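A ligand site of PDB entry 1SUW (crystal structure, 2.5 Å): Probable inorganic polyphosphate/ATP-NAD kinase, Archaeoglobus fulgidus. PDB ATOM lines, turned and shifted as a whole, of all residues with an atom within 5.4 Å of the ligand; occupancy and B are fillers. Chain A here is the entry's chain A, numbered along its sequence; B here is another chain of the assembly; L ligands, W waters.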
ATOM      1  N   GLY A  48      26.426  21.725 -36.802  1.00  0.00           N
ATOM      2  CA  GLY A  48      26.856  22.085 -35.461  1.00  0.00           C
ATOM      3  C   GLY A  48      27.157  20.866 -34.630  1.00  0.00           C
ATOM      4  O   GLY A  48      27.304  19.778 -35.177  1.00  0.00           O
ATOM      5  N   ASP A  49      27.262  21.019 -33.315  1.00  0.00           N
ATOM      6  CA  ASP A  49      27.531  19.874 -32.444  1.00  0.00           C
ATOM      7  C   ASP A  49      26.385  18.869 -32.539  1.00  0.00           C
ATOM      8  O   ASP A  49      26.588  17.665 -32.340  1.00  0.00           O
ATOM      9  CB  ASP A  49      27.704  20.330 -30.995  1.00  0.00           C
ATOM     10  CG  ASP A  49      28.916  21.214 -30.794  1.00  0.00           C
ATOM     11  OD1 ASP A  49      30.011  20.864 -31.282  1.00  0.00           O
ATOM     12  OD2 ASP A  49      28.774  22.276 -30.123  1.00  0.00           O
ATOM     13  N   GLY A  50      25.185  19.355 -32.834  1.00  0.00           N
ATOM     14  CA  GLY A  50      24.044  18.483 -32.944  1.00  0.00           C
ATOM     15  C   GLY A  50      24.205  17.560 -34.129  1.00  0.00           C
ATOM     16  O   GLY A  50      23.895  16.367 -34.070  1.00  0.00           O
ATOM     17  N   THR A  51      24.709  18.117 -35.227  1.00  0.00           N
ATOM     18  CA  THR A  51      24.925  17.328 -36.420  1.00  0.00           C
ATOM     19  C   THR A  51      25.822  16.146 -36.058  1.00  0.00           C
ATOM     20  O   THR A  51      25.566  14.991 -36.412  1.00  0.00           O
ATOM     21  CB  THR A  51      25.621  18.178 -37.500  1.00  0.00           C
ATOM     22  OG1 THR A  51      24.892  19.399 -37.690  1.00  0.00           O
ATOM     23  CG2 THR A  51      25.702  17.422 -38.818  1.00  0.00           C
ATOM     24  N   LEU A  53      26.266  14.784 -33.134  1.00  0.00           N
ATOM     25  CA  LEU A  53      25.600  13.855 -32.245  1.00  0.00           C
ATOM     26  C   LEU A  53      24.682  12.926 -33.035  1.00  0.00           C
ATOM     27  O   LEU A  53      24.635  11.720 -32.782  1.00  0.00           O
ATOM     28  CB  LEU A  53      24.803  14.599 -31.170  1.00  0.00           C
ATOM     29  CG  LEU A  53      25.553  15.404 -30.085  1.00  0.00           C
ATOM     30  CD1 LEU A  53      24.540  16.087 -29.194  1.00  0.00           C
ATOM     31  CD2 LEU A  53      26.451  14.498 -29.259  1.00  0.00           C
ATOM     32  N   ARG A  54      23.962  13.483 -33.995  1.00  0.00           N
ATOM     33  CA  ARG A  54      23.044  12.693 -34.806  1.00  0.00           C
ATOM     34  C   ARG A  54      23.771  11.717 -35.732  1.00  0.00           C
ATOM     35  O   ARG A  54      23.216  10.680 -36.108  1.00  0.00           O
ATOM     36  CB  ARG A  54      22.143  13.620 -35.627  1.00  0.00           C
ATOM     37  CG  ARG A  54      21.095  14.320 -34.771  1.00  0.00           C
ATOM     38  CD  ARG A  54      20.395  15.429 -35.507  1.00  0.00           C
ATOM     39  NE  ARG A  54      19.324  16.029 -34.715  1.00  0.00           N
ATOM     40  CZ  ARG A  54      19.500  16.771 -33.618  1.00  0.00           C
ATOM     41  NH1 ARG A  54      20.725  17.034 -33.168  1.00  0.00           N
ATOM     42  NH2 ARG A  54      18.455  17.264 -32.976  1.00  0.00           N
ATOM     43  N   ASN A  69      31.874  23.912 -38.463  1.00  0.00           N
ATOM     44  CA  ASN A  69      30.823  24.617 -37.735  1.00  0.00           C
ATOM     45  C   ASN A  69      30.051  25.690 -38.491  1.00  0.00           C
ATOM     46  O   ASN A  69      30.603  26.716 -38.885  1.00  0.00           O
ATOM     47  CB  ASN A  69      31.415  25.191 -36.448  1.00  0.00           C
ATOM     48  CG  ASN A  69      30.364  25.811 -35.549  1.00  0.00           C
ATOM     49  OD1 ASN A  69      29.213  25.353 -35.511  1.00  0.00           O
ATOM     50  ND2 ASN A  69      30.744  26.831 -34.801  1.00  0.00           N
ATOM     51  N   GLY A  71      27.079  26.922 -37.102  1.00  0.00           N
ATOM     52  CA  GLY A  71      26.543  27.771 -36.035  1.00  0.00           C
ATOM     53  C   GLY A  71      27.490  28.752 -35.360  1.00  0.00           C
ATOM     54  O   GLY A  71      28.454  29.226 -35.961  1.00  0.00           O
ATOM     55  N   VAL A  73      28.762  28.235 -31.826  1.00  0.00           N
ATOM     56  CA  VAL A  73      29.721  27.550 -30.957  1.00  0.00           C
ATOM     57  C   VAL A  73      29.705  26.051 -31.204  1.00  0.00           C
ATOM     58  O   VAL A  73      28.661  25.407 -31.099  1.00  0.00           O
ATOM     59  CB  VAL A  73      29.425  27.791 -29.460  1.00  0.00           C
ATOM     60  CG1 VAL A  73      30.613  27.332 -28.626  1.00  0.00           C
ATOM     61  CG2 VAL A  73      29.111  29.260 -29.210  1.00  0.00           C
ATOM     62  N   GLY A  74      30.871  25.511 -31.542  1.00  0.00           N
ATOM     63  CA  GLY A  74      30.970  24.090 -31.800  1.00  0.00           C
ATOM     64  C   GLY A  74      32.137  23.456 -31.062  1.00  0.00           C
ATOM     65  O   GLY A  74      33.239  23.385 -31.598  1.00  0.00           O
ATOM     66  N   LEU A  75      31.888  22.997 -29.840  1.00  0.00           N
ATOM     67  CA  LEU A  75      32.939  22.370 -29.054  1.00  0.00           C
ATOM     68  C   LEU A  75      33.447  21.065 -29.662  1.00  0.00           C
ATOM     69  O   LEU A  75      34.528  20.607 -29.315  1.00  0.00           O
ATOM     70  CB  LEU A  75      32.457  22.130 -27.626  1.00  0.00           C
ATOM     71  CG  LEU A  75      32.332  23.347 -26.707  1.00  0.00           C
ATOM     72  CD1 LEU A  75      31.074  24.133 -27.013  1.00  0.00           C
ATOM     73  CD2 LEU A  75      32.314  22.875 -25.267  1.00  0.00           C
ATOM     74  N   LEU A  76      32.667  20.464 -30.559  1.00  0.00           N
ATOM     75  CA  LEU A  76      33.060  19.212 -31.202  1.00  0.00           C
ATOM     76  C   LEU A  76      33.568  19.474 -32.616  1.00  0.00           C
ATOM     77  O   LEU A  76      33.950  18.560 -33.334  1.00  0.00           O
ATOM     78  CB  LEU A  76      31.870  18.247 -31.275  1.00  0.00           C
ATOM     79  CG  LEU A  76      31.118  18.001 -29.976  1.00  0.00           C
ATOM     80  CD1 LEU A  76      29.965  17.035 -30.213  1.00  0.00           C
ATOM     81  CD2 LEU A  76      32.062  17.450 -28.928  1.00  0.00           C
ATOM     82  N   ASN A 115      27.349  12.680 -24.942  1.00  0.00           N
ATOM     83  CA  ASN A 115      27.047  13.751 -24.008  1.00  0.00           C
ATOM     84  C   ASN A 115      26.506  13.236 -22.684  1.00  0.00           C
ATOM     85  O   ASN A 115      27.141  13.384 -21.640  1.00  0.00           O
ATOM     86  CB  ASN A 115      26.048  14.722 -24.628  1.00  0.00           C
ATOM     87  CG  ASN A 115      26.707  15.770 -25.475  1.00  0.00           C
ATOM     88  OD1 ASN A 115      27.927  15.830 -25.591  1.00  0.00           O
ATOM     89  ND2 ASN A 115      25.898  16.629 -26.077  1.00  0.00           N
ATOM     90  N   GLU A 116      25.331  12.624 -22.736  1.00  0.00           N
ATOM     91  CA  GLU A 116      24.739  12.118 -21.501  1.00  0.00           C
ATOM     92  C   GLU A 116      23.529  11.221 -21.684  1.00  0.00           C
ATOM     93  O   GLU A 116      22.946  11.115 -22.763  1.00  0.00           O
ATOM     94  CB  GLU A 116      24.324  13.278 -20.602  1.00  0.00           C
ATOM     95  CG  GLU A 116      23.015  13.938 -21.016  1.00  0.00           C
ATOM     96  CD  GLU A 116      23.124  14.711 -22.325  1.00  0.00           C
ATOM     97  OE1 GLU A 116      23.881  15.697 -22.370  1.00  0.00           O
ATOM     98  OE2 GLU A 116      22.466  14.325 -23.306  1.00  0.00           O
ATOM     99  N   ILE A 153      32.553  15.322 -21.876  1.00  0.00           N
ATOM    100  CA  ILE A 153      32.177  15.981 -23.119  1.00  0.00           C
ATOM    101  C   ILE A 153      30.803  16.617 -22.964  1.00  0.00           C
ATOM    102  O   ILE A 153      30.531  17.695 -23.512  1.00  0.00           O
ATOM    103  CB  ILE A 153      32.153  14.989 -24.310  1.00  0.00           C
ATOM    104  CG1 ILE A 153      33.559  14.417 -24.527  1.00  0.00           C
ATOM    105  CG2 ILE A 153      31.665  15.696 -25.564  1.00  0.00           C
ATOM    106  CD1 ILE A 153      34.616  15.473 -24.801  1.00  0.00           C
ATOM    107  N   GLY A 154      29.945  15.949 -22.196  1.00  0.00           N
ATOM    108  CA  GLY A 154      28.614  16.449 -21.961  1.00  0.00           C
ATOM    109  C   GLY A 154      28.596  17.530 -20.890  1.00  0.00           C
ATOM    110  O   GLY A 154      27.569  18.188 -20.711  1.00  0.00           O
ATOM    111  N   THR A 156      29.509  20.355 -20.935  1.00  0.00           N
ATOM    112  CA  THR A 156      29.208  21.675 -21.489  1.00  0.00           C
ATOM    113  C   THR A 156      27.803  21.703 -22.088  1.00  0.00           C
ATOM    114  O   THR A 156      27.365  22.720 -22.605  1.00  0.00           O
ATOM    115  CB  THR A 156      30.227  22.079 -22.593  1.00  0.00           C
ATOM    116  OG1 THR A 156      30.375  21.008 -23.531  1.00  0.00           O
ATOM    117  CG2 THR A 156      31.580  22.391 -21.976  1.00  0.00           C
ATOM    118  N   GLY A 157      27.107  20.569 -22.002  1.00  0.00           N
ATOM    119  CA  GLY A 157      25.751  20.484 -22.521  1.00  0.00           C
ATOM    120  C   GLY A 157      24.655  20.644 -21.468  1.00  0.00           C
ATOM    121  O   GLY A 157      24.624  21.646 -20.751  1.00  0.00           O
ATOM    122  N   TYR A 158      23.760  19.667 -21.373  1.00  0.00           N
ATOM    123  CA  TYR A 158      22.650  19.684 -20.410  1.00  0.00           C
ATOM    124  C   TYR A 158      23.184  19.890 -18.974  1.00  0.00           C
ATOM    125  O   TYR A 158      22.677  20.732 -18.218  1.00  0.00           O
ATOM    126  CB  TYR A 158      21.869  18.373 -20.493  1.00  0.00           C
ATOM    127  CG  TYR A 158      20.365  18.461 -20.251  1.00  0.00           C
ATOM    128  CD1 TYR A 158      19.784  19.569 -19.612  1.00  0.00           C
ATOM    129  CD2 TYR A 158      19.518  17.418 -20.648  1.00  0.00           C
ATOM    130  CE1 TYR A 158      18.395  19.638 -19.383  1.00  0.00           C
ATOM    131  CE2 TYR A 158      18.133  17.473 -20.418  1.00  0.00           C
ATOM    132  CZ  TYR A 158      17.582  18.583 -19.787  1.00  0.00           C
ATOM    133  OH  TYR A 158      16.212  18.626 -19.578  1.00  0.00           O
ATOM    134  N   ALA A 159      24.200  19.120 -18.591  1.00  0.00           N
ATOM    135  CA  ALA A 159      24.789  19.224 -17.250  1.00  0.00           C
ATOM    136  C   ALA A 159      25.208  20.672 -16.976  1.00  0.00           C
ATOM    137  O   ALA A 159      25.090  21.153 -15.852  1.00  0.00           O
ATOM    138  CB  ALA A 159      25.985  18.282 -17.128  1.00  0.00           C
ATOM    139  N   SER A 161      23.820  23.510 -18.103  1.00  0.00           N
ATOM    140  CA  SER A 161      22.600  24.256 -17.767  1.00  0.00           C
ATOM    141  C   SER A 161      22.005  23.868 -16.419  1.00  0.00           C
ATOM    142  O   SER A 161      21.297  24.650 -15.799  1.00  0.00           O
ATOM    143  CB  SER A 161      21.537  24.047 -18.849  1.00  0.00           C
ATOM    144  OG  SER A 161      22.012  24.472 -20.121  1.00  0.00           O
ATOM    145  N   ASP A 209      21.830  11.496 -25.613  1.00  0.00           N
ATOM    146  CA  ASP A 209      22.267  12.598 -26.456  1.00  0.00           C
ATOM    147  C   ASP A 209      21.088  13.356 -27.054  1.00  0.00           C
ATOM    148  O   ASP A 209      21.196  13.962 -28.124  1.00  0.00           O
ATOM    149  CB  ASP A 209      23.179  12.091 -27.576  1.00  0.00           C
ATOM    150  CG  ASP A 209      24.566  11.710 -27.085  1.00  0.00           C
ATOM    151  OD1 ASP A 209      24.905  12.039 -25.924  1.00  0.00           O
ATOM    152  OD2 ASP A 209      25.327  11.088 -27.854  1.00  0.00           O
ATOM    153  N   GLY A 210      19.955  13.304 -26.355  1.00  0.00           N
ATOM    154  CA  GLY A 210      18.749  13.976 -26.807  1.00  0.00           C
ATOM    155  C   GLY A 210      18.210  13.503 -28.142  1.00  0.00           C
ATOM    156  O   GLY A 210      17.507  14.240 -28.820  1.00  0.00           O
ATOM    157  N   GLN A 211      18.529  12.256 -28.515  1.00  0.00           N
ATOM    158  CA  GLN A 211      18.079  11.702 -29.789  1.00  0.00           C
ATOM    159  C   GLN A 211      17.128  10.528 -29.631  1.00  0.00           C
ATOM    160  O   GLN A 211      16.004  10.556 -30.145  1.00  0.00           O
ATOM    161  CB  GLN A 211      19.268  11.259 -30.634  1.00  0.00           C
ATOM    162  CG  GLN A 211      20.229  12.376 -31.010  1.00  0.00           C
ATOM    163  CD  GLN A 211      19.533  13.682 -31.291  1.00  0.00           C
ATOM    164  OE1 GLN A 211      18.615  13.761 -32.129  1.00  0.00           O
ATOM    165  NE2 GLN A 211      19.941  14.729 -30.586  1.00  0.00           N
ATOM    166  N   ILE A 248      28.580  30.480 -24.779  1.00  0.00           N
ATOM    167  CA  ILE A 248      27.410  29.607 -24.899  1.00  0.00           C
ATOM    168  C   ILE A 248      26.067  30.324 -24.672  1.00  0.00           C
ATOM    169  O   ILE A 248      25.934  31.161 -23.772  1.00  0.00           O
ATOM    170  CB  ILE A 248      27.502  28.412 -23.905  1.00  0.00           C
ATOM    171  CG1 ILE A 248      28.541  27.403 -24.392  1.00  0.00           C
ATOM    172  CG2 ILE A 248      26.128  27.772 -23.740  1.00  0.00           C
ATOM    173  CD1 ILE A 248      28.776  26.241 -23.420  1.00  0.00           C
ATOM    174  N   GLY A 249      25.095  29.988 -25.522  1.00  0.00           N
ATOM    175  CA  GLY A 249      23.767  30.567 -25.435  1.00  0.00           C
ATOM    176  C   GLY A 249      22.810  29.929 -26.436  1.00  0.00           C
ATOM    177  O   GLY A 249      21.748  30.529 -26.727  1.00  0.00           O
ATOM    178  OXT GLY A 249      23.114  28.815 -26.944  1.00  0.00           O
ATOM    179  N   ALA B 125      12.946  16.925 -22.142  1.00  0.00           N
ATOM    180  CA  ALA B 125      14.291  16.968 -22.695  1.00  0.00           C
ATOM    181  C   ALA B 125      14.436  17.884 -23.917  1.00  0.00           C
ATOM    182  O   ALA B 125      15.402  17.766 -24.656  1.00  0.00           O
ATOM    183  CB  ALA B 125      14.751  15.548 -23.061  1.00  0.00           C
ATOM    184  N   LYS B 126      13.466  18.759 -24.128  1.00  0.00           N
ATOM    185  CA  LYS B 126      13.534  19.689 -25.249  1.00  0.00           C
ATOM    186  C   LYS B 126      13.519  21.103 -24.718  1.00  0.00           C
ATOM    187  O   LYS B 126      12.748  21.421 -23.830  1.00  0.00           O
ATOM    188  CB  LYS B 126      12.355  19.470 -26.207  1.00  0.00           C
ATOM    189  CG  LYS B 126      12.726  18.678 -27.461  1.00  0.00           C
ATOM    190  CD  LYS B 126      13.342  17.324 -27.114  1.00  0.00           C
ATOM    191  CE  LYS B 126      13.872  16.594 -28.348  1.00  0.00           C
ATOM    192  NZ  LYS B 126      14.994  17.325 -29.012  1.00  0.00           N
ATOM    193  N   MET B 127      14.397  21.934 -25.248  1.00  0.00           N
ATOM    194  CA  MET B 127      14.457  23.326 -24.823  1.00  0.00           C
ATOM    195  C   MET B 127      13.418  24.152 -25.561  1.00  0.00           C
ATOM    196  O   MET B 127      12.756  23.674 -26.463  1.00  0.00           O
ATOM    197  CB  MET B 127      15.822  23.939 -25.123  1.00  0.00           C
ATOM    198  CG  MET B 127      16.947  23.457 -24.245  1.00  0.00           C
ATOM    199  SD  MET B 127      18.461  24.396 -24.529  1.00  0.00           S
ATOM    200  CE  MET B 127      19.215  23.452 -25.837  1.00  0.00           C
ATOM    201  N   ARG B 143      17.369  30.321 -23.823  1.00  0.00           N
ATOM    202  CA  ARG B 143      17.016  28.941 -24.137  1.00  0.00           C
ATOM    203  C   ARG B 143      17.057  28.181 -22.826  1.00  0.00           C
ATOM    204  O   ARG B 143      18.046  28.224 -22.122  1.00  0.00           O
ATOM    205  CB  ARG B 143      18.022  28.352 -25.125  1.00  0.00           C
ATOM    206  CG  ARG B 143      18.130  29.164 -26.418  1.00  0.00           C
ATOM    207  CD  ARG B 143      19.265  28.649 -27.309  1.00  0.00           C
ATOM    208  NE  ARG B 143      18.943  27.354 -27.907  1.00  0.00           N
ATOM    209  CZ  ARG B 143      19.851  26.541 -28.435  1.00  0.00           C
ATOM    210  NH1 ARG B 143      21.137  26.879 -28.434  1.00  0.00           N
ATOM    211  NH2 ARG B 143      19.473  25.381 -28.969  1.00  0.00           N
ATOM    212  N   CYS B 144      15.970  27.489 -22.503  1.00  0.00           N
ATOM    213  CA  CYS B 144      15.878  26.762 -21.228  1.00  0.00           C
ATOM    214  C   CYS B 144      14.820  25.672 -21.308  1.00  0.00           C
ATOM    215  O   CYS B 144      14.100  25.578 -22.289  1.00  0.00           O
ATOM    216  CB  CYS B 144      15.472  27.760 -20.154  1.00  0.00           C
ATOM    217  SG  CYS B 144      14.024  28.764 -20.661  1.00  0.00           S
ATOM    218  N   ASP B 145      14.722  24.855 -20.253  1.00  0.00           N
ATOM    219  CA  ASP B 145      13.724  23.801 -20.186  1.00  0.00           C
ATOM    220  C   ASP B 145      12.351  24.424 -19.908  1.00  0.00           C
ATOM    221  O   ASP B 145      11.306  23.819 -20.188  1.00  0.00           O
ATOM    222  CB  ASP B 145      14.043  22.791 -19.080  1.00  0.00           C
ATOM    223  CG  ASP B 145      14.951  21.649 -19.545  1.00  0.00           C
ATOM    224  OD1 ASP B 145      15.084  20.655 -18.808  1.00  0.00           O
ATOM    225  OD2 ASP B 145      15.536  21.750 -20.641  1.00  0.00           O
ATOM    226  N   ALA B 180      16.919  25.223 -15.956  1.00  0.00           N
ATOM    227  CA  ALA B 180      17.975  24.673 -16.816  1.00  0.00           C
ATOM    228  C   ALA B 180      18.286  25.611 -17.980  1.00  0.00           C
ATOM    229  O   ALA B 180      18.104  25.262 -19.142  1.00  0.00           O
ATOM    230  CB  ALA B 180      17.581  23.294 -17.351  1.00  0.00           C
ATOM    231  N   PRO B 181      18.747  26.823 -17.675  1.00  0.00           N
ATOM    232  CA  PRO B 181      19.079  27.790 -18.727  1.00  0.00           C
ATOM    233  C   PRO B 181      20.389  27.393 -19.417  1.00  0.00           C
ATOM    234  O   PRO B 181      21.355  27.013 -18.756  1.00  0.00           O
ATOM    235  CB  PRO B 181      19.183  29.086 -17.949  1.00  0.00           C
ATOM    236  CG  PRO B 181      19.789  28.624 -16.646  1.00  0.00           C
ATOM    237  CD  PRO B 181      19.029  27.362 -16.331  1.00  0.00           C
ATOM    238  N   PHE B 182      20.425  27.487 -20.744  1.00  0.00           N
ATOM    239  CA  PHE B 182      21.640  27.146 -21.496  1.00  0.00           C
ATOM    240  C   PHE B 182      22.374  28.423 -21.914  1.00  0.00           C
ATOM    241  O   PHE B 182      22.251  28.891 -23.041  1.00  0.00           O
ATOM    242  CB  PHE B 182      21.281  26.298 -22.719  1.00  0.00           C
ATOM    243  CG  PHE B 182      22.473  25.794 -23.480  1.00  0.00           C
ATOM    244  CD1 PHE B 182      23.515  25.140 -22.829  1.00  0.00           C
ATOM    245  CD2 PHE B 182      22.565  25.967 -24.860  1.00  0.00           C
ATOM    246  CE1 PHE B 182      24.625  24.669 -23.532  1.00  0.00           C
ATOM    247  CE2 PHE B 182      23.671  25.501 -25.570  1.00  0.00           C
ATOM    248  CZ  PHE B 182      24.704  24.845 -24.914  1.00  0.00           C
HETATM  249  P1  LIG L   1      20.125  20.612 -30.301  1.00  0.00           P
HETATM  250  O1  LIG L   1      19.014  21.141 -30.986  1.00  0.00           O
HETATM  251  O2  LIG L   1      20.879  19.318 -30.205  1.00  0.00           O
HETATM  252  O3  LIG L   1      20.291  21.402 -28.903  1.00  0.00           O
HETATM  253  C1  LIG L   1      21.490  21.209 -28.117  1.00  0.00           C
HETATM  254  C2  LIG L   1      22.233  22.597 -28.153  1.00  0.00           C
HETATM  255  O4  LIG L   1      23.435  22.303 -27.345  1.00  0.00           O
HETATM  256  C3  LIG L   1      22.806  22.969 -29.526  1.00  0.00           C
HETATM  257  O5  LIG L   1      22.874  24.410 -29.486  1.00  0.00           O
HETATM  258  C4  LIG L   1      24.189  22.343 -29.576  1.00  0.00           C
HETATM  259  O6  LIG L   1      25.134  22.987 -30.429  1.00  0.00           O
HETATM  260  C5  LIG L   1      24.650  22.398 -28.087  1.00  0.00           C
HETATM  261  N1  LIG L   1      25.460  21.250 -27.720  1.00  0.00           N
HETATM  262  C6  LIG L   1      25.355  19.924 -28.089  1.00  0.00           C
HETATM  263  N2  LIG L   1      26.265  19.142 -27.545  1.00  0.00           N
HETATM  264  C7  LIG L   1      27.011  20.020 -26.772  1.00  0.00           C
HETATM  265  C8  LIG L   1      28.117  19.765 -25.949  1.00  0.00           C
HETATM  266  N3  LIG L   1      28.699  18.563 -25.722  1.00  0.00           N
HETATM  267  N4  LIG L   1      28.667  20.858 -25.285  1.00  0.00           N
HETATM  268  C9  LIG L   1      28.139  22.148 -25.437  1.00  0.00           C
HETATM  269  N5  LIG L   1      27.050  22.423 -26.241  1.00  0.00           N
HETATM  270  C10 LIG L   1      26.521  21.330 -26.891  1.00  0.00           C
HETATM  271  O7  LIG L   1      18.976  19.758 -29.509  1.00  0.00           O
HETATM  272  P2  LIG L   1      18.753  18.253 -28.886  1.00  0.00           P
HETATM  273  O8  LIG L   1      18.316  17.305 -29.936  1.00  0.00           O
HETATM  274  O9  LIG L   1      17.820  18.429 -27.765  1.00  0.00           O
HETATM  275  O10 LIG L   1      20.209  17.801 -28.430  1.00  0.00           O
HETATM  276  C11 LIG L   1      20.386  16.947 -27.254  1.00  0.00           C
HETATM  277  C12 LIG L   1      21.637  17.397 -26.568  1.00  0.00           C
HETATM  278  O11 LIG L   1      21.492  18.783 -26.199  1.00  0.00           O
HETATM  279  C13 LIG L   1      21.979  16.628 -25.268  1.00  0.00           C
HETATM  280  O12 LIG L   1      23.142  15.803 -25.446  1.00  0.00           O
HETATM  281  C14 LIG L   1      22.173  17.684 -24.184  1.00  0.00           C
HETATM  282  O13 LIG L   1      23.507  17.804 -23.710  1.00  0.00           O
HETATM  283  C15 LIG L   1      21.731  18.975 -24.774  1.00  0.00           C
HETATM  284  N6  LIG L   1      20.480  19.531 -24.180  1.00  0.00           N
HETATM  285  C16 LIG L   1      20.524  20.632 -23.305  1.00  0.00           C
HETATM  286  C17 LIG L   1      19.325  21.103 -22.759  1.00  0.00           C
HETATM  287  C18 LIG L   1      19.388  22.296 -21.808  1.00  0.00           C
HETATM  288  O14 LIG L   1      18.348  22.684 -21.332  1.00  0.00           O
HETATM  289  N7  LIG L   1      20.540  22.859 -21.524  1.00  0.00           N
HETATM  290  C19 LIG L   1      18.040  20.485 -23.077  1.00  0.00           C
HETATM  291  C20 LIG L   1      18.033  19.371 -23.976  1.00  0.00           C
HETATM  292  C21 LIG L   1      19.250  18.874 -24.542  1.00  0.00           C
HETATM  293  P3  LIG L   1      24.918  23.239 -32.034  1.00  0.00           P
HETATM  294  O15 LIG L   1      26.278  23.740 -32.542  1.00  0.00           O
HETATM  295  O16 LIG L   1      24.575  21.886 -32.529  1.00  0.00           O
HETATM  296  O17 LIG L   1      23.859  24.299 -32.193  1.00  0.00           O
HETATM  297  O   HOH W   1      16.392  20.706 -27.149  1.00  0.00           O
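OG1 of Thr 156 sits at hydrogen-bond distance from N4 of the ligand, at 2.5 Å.
The side-chain carboxylate (OE1) of Glu 116 lies within hydrogen-bond range of an oxygen (O13) of the ligand.
The side-chain hydroxyl of Ser 161 sits at hydrogen-bond distance from a nitrogen (N7) of the ligand.
The backbone NH (N) of Gly 50 lies within hydrogen-bond range of an oxygen (O16) of the ligand (2.6 Å).
A nitrogen (N3) of the ligand lies within hydrogen-bond range of the side-chain amide oxygen (OD1) of Asn 115.
An oxygen (O16) of the ligand is in hydrogen-bond range of the backbone NH of Asp 49 (2.9 Å).
O of Ile 153 is in hydrogen-bond range of N3 of the ligand (3.0 Å).
The backbone NH (N) of Tyr 158 sits at hydrogen-bond distance from an oxygen (O13) of the ligand (3.0 Å).
An oxygen (O8) of the ligand lies within salt-bridge range of the guanidinium group of Arg 54 (3.0 Å).
O8 of the ligand sits at hydrogen-bond distance from NE2 of Gln 211 (3.1 Å).
The guanidinium group of Arg 143 of chain B is in hydrogen-bond range of an oxygen (O5) of the ligand, 3.2 Å away.
NZ of Lys 126 of chain B is in salt-bridge range of O9 of the ligand (3.3 Å).
The backbone carbonyl oxygen (O) of Val 73 lies close to an oxygen (O15) of the ligand, at 3.2 Å.
O of Gly 210 lies close to O8 of the ligand, 3.4 Å away.
O14 of the ligand sits close to SD of Met 127 of chain B, 3.6 Å away.
O14 of the ligand sits close to OD2 of Asp 145 of chain B, 3.0 Å away.
An oxygen (O14) of the ligand lies close to the backbone carbonyl oxygen of Ala 180 of chain B.
Merely in contact with the ligand: Ala 125 of chain B (3.2 Å), Asp 209 (3.2 Å), Gly 48 (3.4 Å), Phe 182 of chain B (3.6 Å), Gly 157 (3.6 Å), Leu 53 (3.9 Å) and Leu 75 (3.9 Å).
Within 4 Å of the ligand: Gly 48, Asp 49, Gly 50, Leu 53, Arg 54, Val 73, Leu 75, Asn 115, Glu 116, Ile 153, Thr 156, Gly 157, Tyr 158, Ser 161, Asp 209, Gly 210, Gln 211, Ala 125 of chain B, Lys 126 of chain B, Met 127 of chain B, Arg 143 of chain B, Asp 145 of chain B, Ala 180 of chain B and Phe 182 of chain B.
Water W1 lies within hydrogen-bond range of an oxygen (O9) of the ligand and the backbone NH of Met 127 of chain B.
The side-chain hydroxyl (OG1) of Thr 156 lies within hydrogen-bond range of the backbone carbonyl oxygen (O) of Ile 153, at 3.3 Å.
The backbone carbonyl oxygen (O) of Glu 116 lies within hydrogen-bond range of the backbone NH (N) of Asp 209 (3.1 Å).
The backbone NH (N) of Phe 182 of chain B lies close to the side-chain hydroxyl (OG) of Ser 161 (3.5 Å).
N of Leu 75 sits at hydrogen-bond distance from OD1 of Asp 49 (3.2 Å).
The backbone NH of Leu 76 is in hydrogen-bond range of the side-chain carboxylate of Asp 49 (2.8 Å).
The side-chain amide nitrogen (NE2) of Gln 211 sits at hydrogen-bond distance from the backbone carbonyl oxygen (O) of Asp 209 (2.9 Å).
The backbone carbonyl oxygen (O) of Arg 143 of chain B is in hydrogen-bond range of the backbone NH (N) of Phe 182 of chain B (2.8 Å).
The backbone NH (N) of Gly 48 lies within hydrogen-bond range of the side-chain hydroxyl (OG1) of Thr 51 (2.9 Å).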
